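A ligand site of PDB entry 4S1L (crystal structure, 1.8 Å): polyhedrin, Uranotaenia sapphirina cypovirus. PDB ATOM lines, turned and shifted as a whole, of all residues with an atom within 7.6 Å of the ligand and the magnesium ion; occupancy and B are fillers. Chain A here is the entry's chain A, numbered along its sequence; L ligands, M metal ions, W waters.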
ATOM      1  N   ASN A  17     -16.940 -10.514  37.113  1.00  0.00           N
ATOM      2  CA  ASN A  17     -17.335  -9.111  36.947  1.00  0.00           C
ATOM      3  C   ASN A  17     -17.574  -8.404  38.277  1.00  0.00           C
ATOM      4  O   ASN A  17     -17.257  -7.224  38.413  1.00  0.00           O
ATOM      5  CB  ASN A  17     -18.613  -9.008  36.100  1.00  0.00           C
ATOM      6  CG  ASN A  17     -18.385  -9.337  34.628  1.00  0.00           C
ATOM      7  OD1 ASN A  17     -17.253  -9.296  34.136  1.00  0.00           O
ATOM      8  ND2 ASN A  17     -19.457  -9.680  33.938  1.00  0.00           N
ATOM      9  N   ARG A 107      -9.629   1.200  38.250  1.00  0.00           N
ATOM     10  CA  ARG A 107     -10.564   0.097  38.049  1.00  0.00           C
ATOM     11  C   ARG A 107     -11.014  -0.468  39.388  1.00  0.00           C
ATOM     12  O   ARG A 107     -10.163  -0.874  40.186  1.00  0.00           O
ATOM     13  CB  ARG A 107      -9.926  -1.018  37.218  1.00  0.00           C
ATOM     14  CG  ARG A 107     -10.924  -2.024  36.661  1.00  0.00           C
ATOM     15  CD  ARG A 107     -10.276  -3.306  36.149  1.00  0.00           C
ATOM     16  NE  ARG A 107     -11.234  -4.103  35.387  1.00  0.00           N
ATOM     17  CZ  ARG A 107     -12.098  -4.978  35.909  1.00  0.00           C
ATOM     18  NH1 ARG A 107     -12.116  -5.217  37.210  1.00  0.00           N
ATOM     19  NH2 ARG A 107     -12.932  -5.645  35.112  1.00  0.00           N
ATOM     20  N   VAL A 150     -13.071   9.891  32.282  1.00  0.00           N
ATOM     21  CA  VAL A 150     -13.510   9.309  31.017  1.00  0.00           C
ATOM     22  C   VAL A 150     -13.819   7.819  31.201  1.00  0.00           C
ATOM     23  O   VAL A 150     -12.985   7.059  31.644  1.00  0.00           O
ATOM     24  CB  VAL A 150     -12.423   9.497  29.927  1.00  0.00           C
ATOM     25  CG1 VAL A 150     -12.851   8.844  28.606  1.00  0.00           C
ATOM     26  CG2 VAL A 150     -12.105  10.978  29.736  1.00  0.00           C
ATOM     27  N   ASP A 151     -15.031   7.411  30.847  1.00  0.00           N
ATOM     28  CA  ASP A 151     -15.432   6.011  30.997  1.00  0.00           C
ATOM     29  C   ASP A 151     -14.769   5.146  29.940  1.00  0.00           C
ATOM     30  O   ASP A 151     -14.691   5.569  28.799  1.00  0.00           O
ATOM     31  CB  ASP A 151     -16.963   5.833  30.879  1.00  0.00           C
ATOM     32  CG  ASP A 151     -17.743   6.575  31.967  1.00  0.00           C
ATOM     33  OD1 ASP A 151     -17.191   6.918  33.026  1.00  0.00           O
ATOM     34  OD2 ASP A 151     -18.941   6.826  31.737  1.00  0.00           O
ATOM     35  N   LEU A 152     -14.348   3.930  30.307  1.00  0.00           N
ATOM     36  CA  LEU A 152     -13.771   2.980  29.364  1.00  0.00           C
ATOM     37  C   LEU A 152     -14.350   1.607  29.640  1.00  0.00           C
ATOM     38  O   LEU A 152     -14.810   1.353  30.747  1.00  0.00           O
ATOM     39  CB  LEU A 152     -12.227   2.944  29.461  1.00  0.00           C
ATOM     40  CG  LEU A 152     -11.481   4.212  28.984  1.00  0.00           C
ATOM     41  CD1 LEU A 152     -10.006   4.093  29.227  1.00  0.00           C
ATOM     42  CD2 LEU A 152     -11.729   4.496  27.501  1.00  0.00           C
ATOM     43  N   PRO A 153     -14.357   0.710  28.633  1.00  0.00           N
ATOM     44  CA  PRO A 153     -14.860  -0.662  28.856  1.00  0.00           C
ATOM     45  C   PRO A 153     -14.065  -1.438  29.912  1.00  0.00           C
ATOM     46  O   PRO A 153     -12.837  -1.362  29.925  1.00  0.00           O
ATOM     47  CB  PRO A 153     -14.704  -1.328  27.483  1.00  0.00           C
ATOM     48  CG  PRO A 153     -14.668  -0.198  26.509  1.00  0.00           C
ATOM     49  CD  PRO A 153     -13.947   0.909  27.230  1.00  0.00           C
ATOM     50  N   SER A 154     -14.761  -2.183  30.765  1.00  0.00           N
ATOM     51  CA  SER A 154     -14.132  -3.054  31.749  1.00  0.00           C
ATOM     52  C   SER A 154     -14.610  -4.502  31.545  1.00  0.00           C
ATOM     53  O   SER A 154     -14.442  -5.340  32.412  1.00  0.00           O
ATOM     54  CB  SER A 154     -14.439  -2.590  33.190  1.00  0.00           C
ATOM     55  OG  SER A 154     -15.804  -2.703  33.520  1.00  0.00           O
ATOM     56  N   CYS A 155     -15.217  -4.746  30.383  1.00  0.00           N
ATOM     57  CA  CYS A 155     -15.645  -6.078  29.961  1.00  0.00           C
ATOM     58  C   CYS A 155     -16.586  -6.786  30.944  1.00  0.00           C
ATOM     59  O   CYS A 155     -16.454  -7.994  31.210  1.00  0.00           O
ATOM     60  CB  CYS A 155     -14.410  -6.936  29.679  1.00  0.00           C
ATOM     61  SG  CYS A 155     -13.384  -6.234  28.405  1.00  0.00           S
ATOM     62  N   GLY A 156     -17.563  -6.037  31.428  1.00  0.00           N
ATOM     63  CA  GLY A 156     -18.601  -6.581  32.298  1.00  0.00           C
ATOM     64  C   GLY A 156     -18.599  -6.012  33.711  1.00  0.00           C
ATOM     65  O   GLY A 156     -19.581  -6.119  34.414  1.00  0.00           O
ATOM     66  N   GLY A 157     -17.491  -5.392  34.108  1.00  0.00           N
ATOM     67  CA  GLY A 157     -17.349  -4.920  35.470  1.00  0.00           C
ATOM     68  C   GLY A 157     -18.034  -3.595  35.750  1.00  0.00           C
ATOM     69  O   GLY A 157     -18.280  -3.266  36.925  1.00  0.00           O
ATOM     70  N   ARG A 158     -18.368  -2.848  34.700  1.00  0.00           N
ATOM     71  CA  ARG A 158     -18.916  -1.493  34.828  1.00  0.00           C
ATOM     72  C   ARG A 158     -18.069  -0.625  35.775  1.00  0.00           C
ATOM     73  O   ARG A 158     -18.624   0.166  36.571  1.00  0.00           O
ATOM     74  CB  ARG A 158     -20.360  -1.510  35.366  1.00  0.00           C
ATOM     75  CG  ARG A 158     -21.420  -2.004  34.382  1.00  0.00           C
ATOM     76  CD  ARG A 158     -21.973  -3.371  34.745  1.00  0.00           C
ATOM     77  NE  ARG A 158     -22.583  -3.452  36.087  1.00  0.00           N
ATOM     78  CZ  ARG A 158     -22.363  -4.439  36.969  1.00  0.00           C
ATOM     79  NH1 ARG A 158     -21.528  -5.430  36.681  1.00  0.00           N
ATOM     80  NH2 ARG A 158     -22.974  -4.419  38.154  1.00  0.00           N
ATOM     81  N   CYS A 159     -16.751  -0.739  35.713  1.00  0.00           N
ATOM     82  CA  CYS A 159     -15.953  -0.137  36.781  1.00  0.00           C
ATOM     83  C   CYS A 159     -14.562   0.384  36.406  1.00  0.00           C
ATOM     84  O   CYS A 159     -13.683   0.402  37.262  1.00  0.00           O
ATOM     85  CB  CYS A 159     -15.814  -1.147  37.925  1.00  0.00           C
ATOM     86  SG  CYS A 159     -14.841  -2.616  37.522  1.00  0.00           S
ATOM     87  N   GLU A 160     -14.379   0.828  35.159  1.00  0.00           N
ATOM     88  CA  GLU A 160     -13.116   1.484  34.794  1.00  0.00           C
ATOM     89  C   GLU A 160     -13.347   2.889  34.247  1.00  0.00           C
ATOM     90  O   GLU A 160     -14.236   3.123  33.440  1.00  0.00           O
ATOM     91  CB  GLU A 160     -12.330   0.661  33.766  1.00  0.00           C
ATOM     92  CG  GLU A 160     -10.955   1.299  33.512  1.00  0.00           C
ATOM     93  CD  GLU A 160     -10.134   0.611  32.434  1.00  0.00           C
ATOM     94  OE1 GLU A 160     -10.244  -0.611  32.246  1.00  0.00           O
ATOM     95  OE2 GLU A 160      -9.350   1.304  31.784  1.00  0.00           O
ATOM     96  N   THR A 228      -8.164  -1.913  30.410  1.00  0.00           N
ATOM     97  CA  THR A 228      -8.369  -1.407  29.056  1.00  0.00           C
ATOM     98  C   THR A 228      -7.671  -0.065  28.963  1.00  0.00           C
ATOM     99  O   THR A 228      -7.788   0.770  29.863  1.00  0.00           O
ATOM    100  CB  THR A 228      -9.889  -1.268  28.725  1.00  0.00           C
ATOM    101  OG1 THR A 228     -10.528  -2.545  28.911  1.00  0.00           O
ATOM    102  CG2 THR A 228     -10.085  -0.787  27.295  1.00  0.00           C
ATOM    103  N   MET A 229      -6.945   0.163  27.876  1.00  0.00           N
ATOM    104  CA  MET A 229      -6.236   1.417  27.692  1.00  0.00           C
ATOM    105  C   MET A 229      -6.628   2.040  26.356  1.00  0.00           C
ATOM    106  O   MET A 229      -7.065   1.342  25.453  1.00  0.00           O
ATOM    107  CB  MET A 229      -4.739   1.208  27.768  1.00  0.00           C
ATOM    108  CG  MET A 229      -4.260   0.938  29.186  1.00  0.00           C
ATOM    109  SD  MET A 229      -2.485   0.739  29.233  1.00  0.00           S
ATOM    110  CE  MET A 229      -2.237   0.182  30.898  1.00  0.00           C
ATOM    111  N   LEU A 230      -6.489   3.359  26.278  1.00  0.00           N
ATOM    112  CA  LEU A 230      -6.910   4.146  25.119  1.00  0.00           C
ATOM    113  C   LEU A 230      -5.680   4.742  24.472  1.00  0.00           C
ATOM    114  O   LEU A 230      -4.851   5.331  25.173  1.00  0.00           O
ATOM    115  CB  LEU A 230      -7.861   5.261  25.555  1.00  0.00           C
ATOM    116  CG  LEU A 230      -8.656   5.950  24.451  1.00  0.00           C
ATOM    117  CD1 LEU A 230      -9.663   4.982  23.877  1.00  0.00           C
ATOM    118  CD2 LEU A 230      -9.357   7.189  25.014  1.00  0.00           C
ATOM    119  N   ASP A 231      -5.526   4.610  23.149  1.00  0.00           N
ATOM    120  CA  ASP A 231      -4.346   5.195  22.484  1.00  0.00           C
ATOM    121  C   ASP A 231      -4.642   6.585  21.887  1.00  0.00           C
ATOM    122  O   ASP A 231      -5.742   7.121  22.046  1.00  0.00           O
ATOM    123  CB  ASP A 231      -3.779   4.224  21.418  1.00  0.00           C
ATOM    124  CG  ASP A 231      -4.703   4.002  20.236  1.00  0.00           C
ATOM    125  OD1 ASP A 231      -5.604   4.844  20.018  1.00  0.00           O
ATOM    126  OD2 ASP A 231      -4.528   2.970  19.518  1.00  0.00           O
ATOM    127  N   PHE A 233      -5.285   7.447  18.988  1.00  0.00           N
ATOM    128  CA  PHE A 233      -6.319   7.389  17.936  1.00  0.00           C
ATOM    129  C   PHE A 233      -7.696   7.073  18.504  1.00  0.00           C
ATOM    130  O   PHE A 233      -8.636   6.779  17.752  1.00  0.00           O
ATOM    131  CB  PHE A 233      -5.916   6.336  16.893  1.00  0.00           C
ATOM    132  CG  PHE A 233      -4.484   6.454  16.473  1.00  0.00           C
ATOM    133  CD1 PHE A 233      -4.072   7.528  15.691  1.00  0.00           C
ATOM    134  CD2 PHE A 233      -3.553   5.525  16.899  1.00  0.00           C
ATOM    135  CE1 PHE A 233      -2.756   7.658  15.318  1.00  0.00           C
ATOM    136  CE2 PHE A 233      -2.220   5.649  16.540  1.00  0.00           C
ATOM    137  CZ  PHE A 233      -1.816   6.719  15.737  1.00  0.00           C
ATOM    138  N   SER A 234      -7.799   7.127  19.821  1.00  0.00           N
ATOM    139  CA  SER A 234      -9.009   6.751  20.553  1.00  0.00           C
ATOM    140  C   SER A 234      -9.448   5.331  20.238  1.00  0.00           C
ATOM    141  O   SER A 234     -10.646   5.051  20.166  1.00  0.00           O
ATOM    142  CB  SER A 234     -10.158   7.727  20.265  1.00  0.00           C
ATOM    143  OG  SER A 234     -11.153   7.595  21.277  1.00  0.00           O
ATOM    144  N   VAL A 235      -8.482   4.439  20.063  1.00  0.00           N
ATOM    145  CA  VAL A 235      -8.756   3.009  19.934  1.00  0.00           C
ATOM    146  C   VAL A 235      -8.382   2.321  21.245  1.00  0.00           C
ATOM    147  O   VAL A 235      -7.323   2.628  21.830  1.00  0.00           O
ATOM    148  CB  VAL A 235      -7.975   2.381  18.749  1.00  0.00           C
ATOM    149  CG1 VAL A 235      -8.107   0.880  18.723  1.00  0.00           C
ATOM    150  CG2 VAL A 235      -8.454   3.005  17.421  1.00  0.00           C
ATOM    151  N   ILE A 236      -9.224   1.382  21.687  1.00  0.00           N
ATOM    152  CA  ILE A 236      -8.995   0.688  22.952  1.00  0.00           C
ATOM    153  C   ILE A 236      -8.166  -0.577  22.747  1.00  0.00           C
ATOM    154  O   ILE A 236      -8.212  -1.220  21.688  1.00  0.00           O
ATOM    155  CB  ILE A 236     -10.322   0.320  23.689  1.00  0.00           C
ATOM    156  CG1 ILE A 236     -11.186  -0.648  22.843  1.00  0.00           C
ATOM    157  CG2 ILE A 236     -11.077   1.595  24.068  1.00  0.00           C
ATOM    158  CD1 ILE A 236     -12.493  -1.063  23.503  1.00  0.00           C
ATOM    159  N   HIS A 237      -7.414  -0.922  23.789  1.00  0.00           N
ATOM    160  CA  HIS A 237      -6.558  -2.105  23.812  1.00  0.00           C
ATOM    161  C   HIS A 237      -6.724  -2.829  25.134  1.00  0.00           C
ATOM    162  O   HIS A 237      -6.985  -2.148  26.134  1.00  0.00           O
ATOM    163  CB  HIS A 237      -5.111  -1.704  23.615  1.00  0.00           C
ATOM    164  CG  HIS A 237      -4.890  -0.902  22.380  1.00  0.00           C
ATOM    165  ND1 HIS A 237      -4.619  -1.480  21.156  1.00  0.00           N
ATOM    166  CD2 HIS A 237      -5.008   0.429  22.146  1.00  0.00           C
ATOM    167  CE1 HIS A 237      -4.543  -0.538  20.237  1.00  0.00           C
ATOM    168  NE2 HIS A 237      -4.766   0.625  20.817  1.00  0.00           N
ATOM    169  OXT HIS A 237      -6.599  -4.055  25.231  1.00  0.00           O
HETATM  170  P1  LIG L   1     -18.402  -2.105  31.103  1.00  0.00           P
HETATM  171  O1  LIG L   1     -17.315  -1.353  31.825  1.00  0.00           O
HETATM  172  O2  LIG L   1     -19.575  -1.271  30.660  1.00  0.00           O
HETATM  173  O3  LIG L   1     -18.821  -3.375  31.844  1.00  0.00           O
HETATM  174  P2  LIG L   1     -18.236  -3.012  28.397  1.00  0.00           P
HETATM  175  O4  LIG L   1     -17.269  -4.031  27.818  1.00  0.00           O
HETATM  176  O5  LIG L   1     -19.683  -3.385  28.570  1.00  0.00           O
HETATM  177  O6  LIG L   1     -17.599  -2.518  29.787  1.00  0.00           O
HETATM  178  P3  LIG L   1     -19.187  -0.694  26.932  1.00  0.00           P
HETATM  179  O7  LIG L   1     -19.256  -1.055  25.466  1.00  0.00           O
HETATM  180  O8  LIG L   1     -20.466  -0.693  27.752  1.00  0.00           O
HETATM  181  O9  LIG L   1     -18.035  -1.664  27.537  1.00  0.00           O
HETATM  182  O10 LIG L   1     -18.435   0.731  27.056  1.00  0.00           O
HETATM  183  C1  LIG L   1     -18.186   1.360  28.327  1.00  0.00           C
HETATM  184  C2  LIG L   1     -17.794   2.804  28.056  1.00  0.00           C
HETATM  185  O11 LIG L   1     -16.571   2.850  27.311  1.00  0.00           O
HETATM  186  C3  LIG L   1     -18.829   3.544  27.208  1.00  0.00           C
HETATM  187  O12 LIG L   1     -19.037   4.844  27.768  1.00  0.00           O
HETATM  188  C4  LIG L   1     -18.160   3.726  25.865  1.00  0.00           C
HETATM  189  O13 LIG L   1     -18.551   4.904  25.165  1.00  0.00           O
HETATM  190  C5  LIG L   1     -16.694   3.806  26.247  1.00  0.00           C
HETATM  191  N1  LIG L   1     -15.868   3.498  25.059  1.00  0.00           N
HETATM  192  C6  LIG L   1     -15.946   2.332  24.395  1.00  0.00           C
HETATM  193  N2  LIG L   1     -15.087   2.333  23.340  1.00  0.00           N
HETATM  194  C7  LIG L   1     -14.461   3.519  23.339  1.00  0.00           C
HETATM  195  C8  LIG L   1     -13.438   4.142  22.476  1.00  0.00           C
HETATM  196  N3  LIG L   1     -12.973   3.403  21.443  1.00  0.00           N
HETATM  197  N4  LIG L   1     -13.040   5.405  22.785  1.00  0.00           N
HETATM  198  C9  LIG L   1     -13.555   6.075  23.848  1.00  0.00           C
HETATM  199  N5  LIG L   1     -14.493   5.550  24.658  1.00  0.00           N
HETATM  200  C10 LIG L   1     -14.979   4.296  24.463  1.00  0.00           C
HETATM  201 MG    MG M   1     -20.960  -2.040  29.265  1.00  0.00          MG
HETATM  202  O   HOH W   1     -22.322  -0.470  30.239  1.00  0.00           O
HETATM  203  O   HOH W   2     -16.335   0.843  32.855  1.00  0.00           O
HETATM  204  O   HOH W   3     -11.748   1.054  19.844  1.00  0.00           O
HETATM  205  O   HOH W   4     -15.516   7.271  26.708  1.00  0.00           O
HETATM  206  O   HOH W   5     -22.610  -2.738  27.774  1.00  0.00           O
HETATM  207  O   HOH W   6     -21.317  -3.587  30.963  1.00  0.00           O
HETATM  208  O   HOH W   7     -22.170   1.436  27.774  1.00  0.00           O
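The side-chain hydroxyl (OG) of Ser 234 lies within hydrogen-bond range of a nitrogen (N4) of the ligand, 3.3 Å away. N of Gly 156 lies within hydrogen-bond range of O3 of the ligand (3.0 Å). O1 of the ligand sits at hydrogen-bond distance from OG of Ser 154. An oxygen (O3) of the ligand lies within hydrogen-bond range of the backbone NH (N) of Arg 158, 2.9 Å away. An oxygen (O6) of the ligand is in hydrogen-bond range of the backbone NH (N) of Cys 155 (3.3 Å). The backbone carbonyl oxygen (O) of Ser 234 lies within hydrogen-bond range of a nitrogen (N3) of the ligand, at 3.1 Å. The backbone NH of Gly 157 is in hydrogen-bond range of an oxygen (O3) of the ligand (3.3 Å). O1 of the ligand is in hydrogen-bond range of N of Ser 154 (2.9 Å).
N of Ser 234 sits at hydrogen-bond distance from OD1 of Asp 231. N of Cys 159 sits at hydrogen-bond distance from OG of Ser 154. The backbone carbonyl oxygen (O) of Gly 156 is in hydrogen-bond range of the guanidinium group (NH1) of Arg 158 (3.1 Å). N of Arg 158 is in hydrogen-bond range of OG of Ser 154 (2.8 Å). O of Gly 157 lies close to SG of Cys 159 (3.6 Å). The side-chain amide oxygen (OD1) of Asn 17 lies close to the backbone carbonyl oxygen (O) of Cys 155, 3.3 Å away. O of Ser 154 sits at hydrogen-bond distance from NH2 of Arg 107, 3.1 Å away. The backbone carbonyl oxygen of Pro 153 is in hydrogen-bond range of the side-chain hydroxyl of Thr 228 (2.8 Å).
N of Pro 153 sits close to O11 of the ligand. Asp 151 touches the ligand (O to O11, 3.6 Å). Leu 152 touches the ligand (C to O11, 3.4 Å). N of Cys 159 touches O1 of the ligand (3.98 Å). CD1 of Leu 230 touches N4 of the ligand (3.6 Å). Ile 236 touches the ligand. Within 4 Å of the ligand: Asp 151, Leu 152, Pro 153, Ser 154, Cys 155, Gly 156, Gly 157, Arg 158, Cys 159, Leu 230, Ser 234 and Ile 236. The nearest printed residue that does not touch the ligand is Val 235 (4.5 Å).
No residue comes within 4 Å of the magnesium ion.
The magnesium ion is bound by an oxygen (O5) of the ligand (2.0 Å), an oxygen (O8) of the ligand (2.1 Å), an oxygen (O2) of the ligand (2.1 Å), water W1 (2.3 Å), water W6 (2.3 Å) and water W5 (2.3 Å). The magnesium ion has six donor atoms within binding distance.
Water W2 lies within hydrogen-bond range of an oxygen (O1) of the ligand (2.6 Å), the backbone carbonyl oxygen of Leu 152 (2.7 Å), the backbone NH of Glu 160 (3.0 Å) and the backbone NH of Cys 159 (3.3 Å). Water W4 lies within hydrogen-bond range of the backbone carbonyl oxygen (O) of Asp 151 (2.8 Å) and a nitrogen (N5) of the ligand (2.9 Å). Water W3 lies within hydrogen-bond range of a nitrogen (N3) of the ligand (3.1 Å) and the backbone NH of Ile 236 (3.1 Å).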
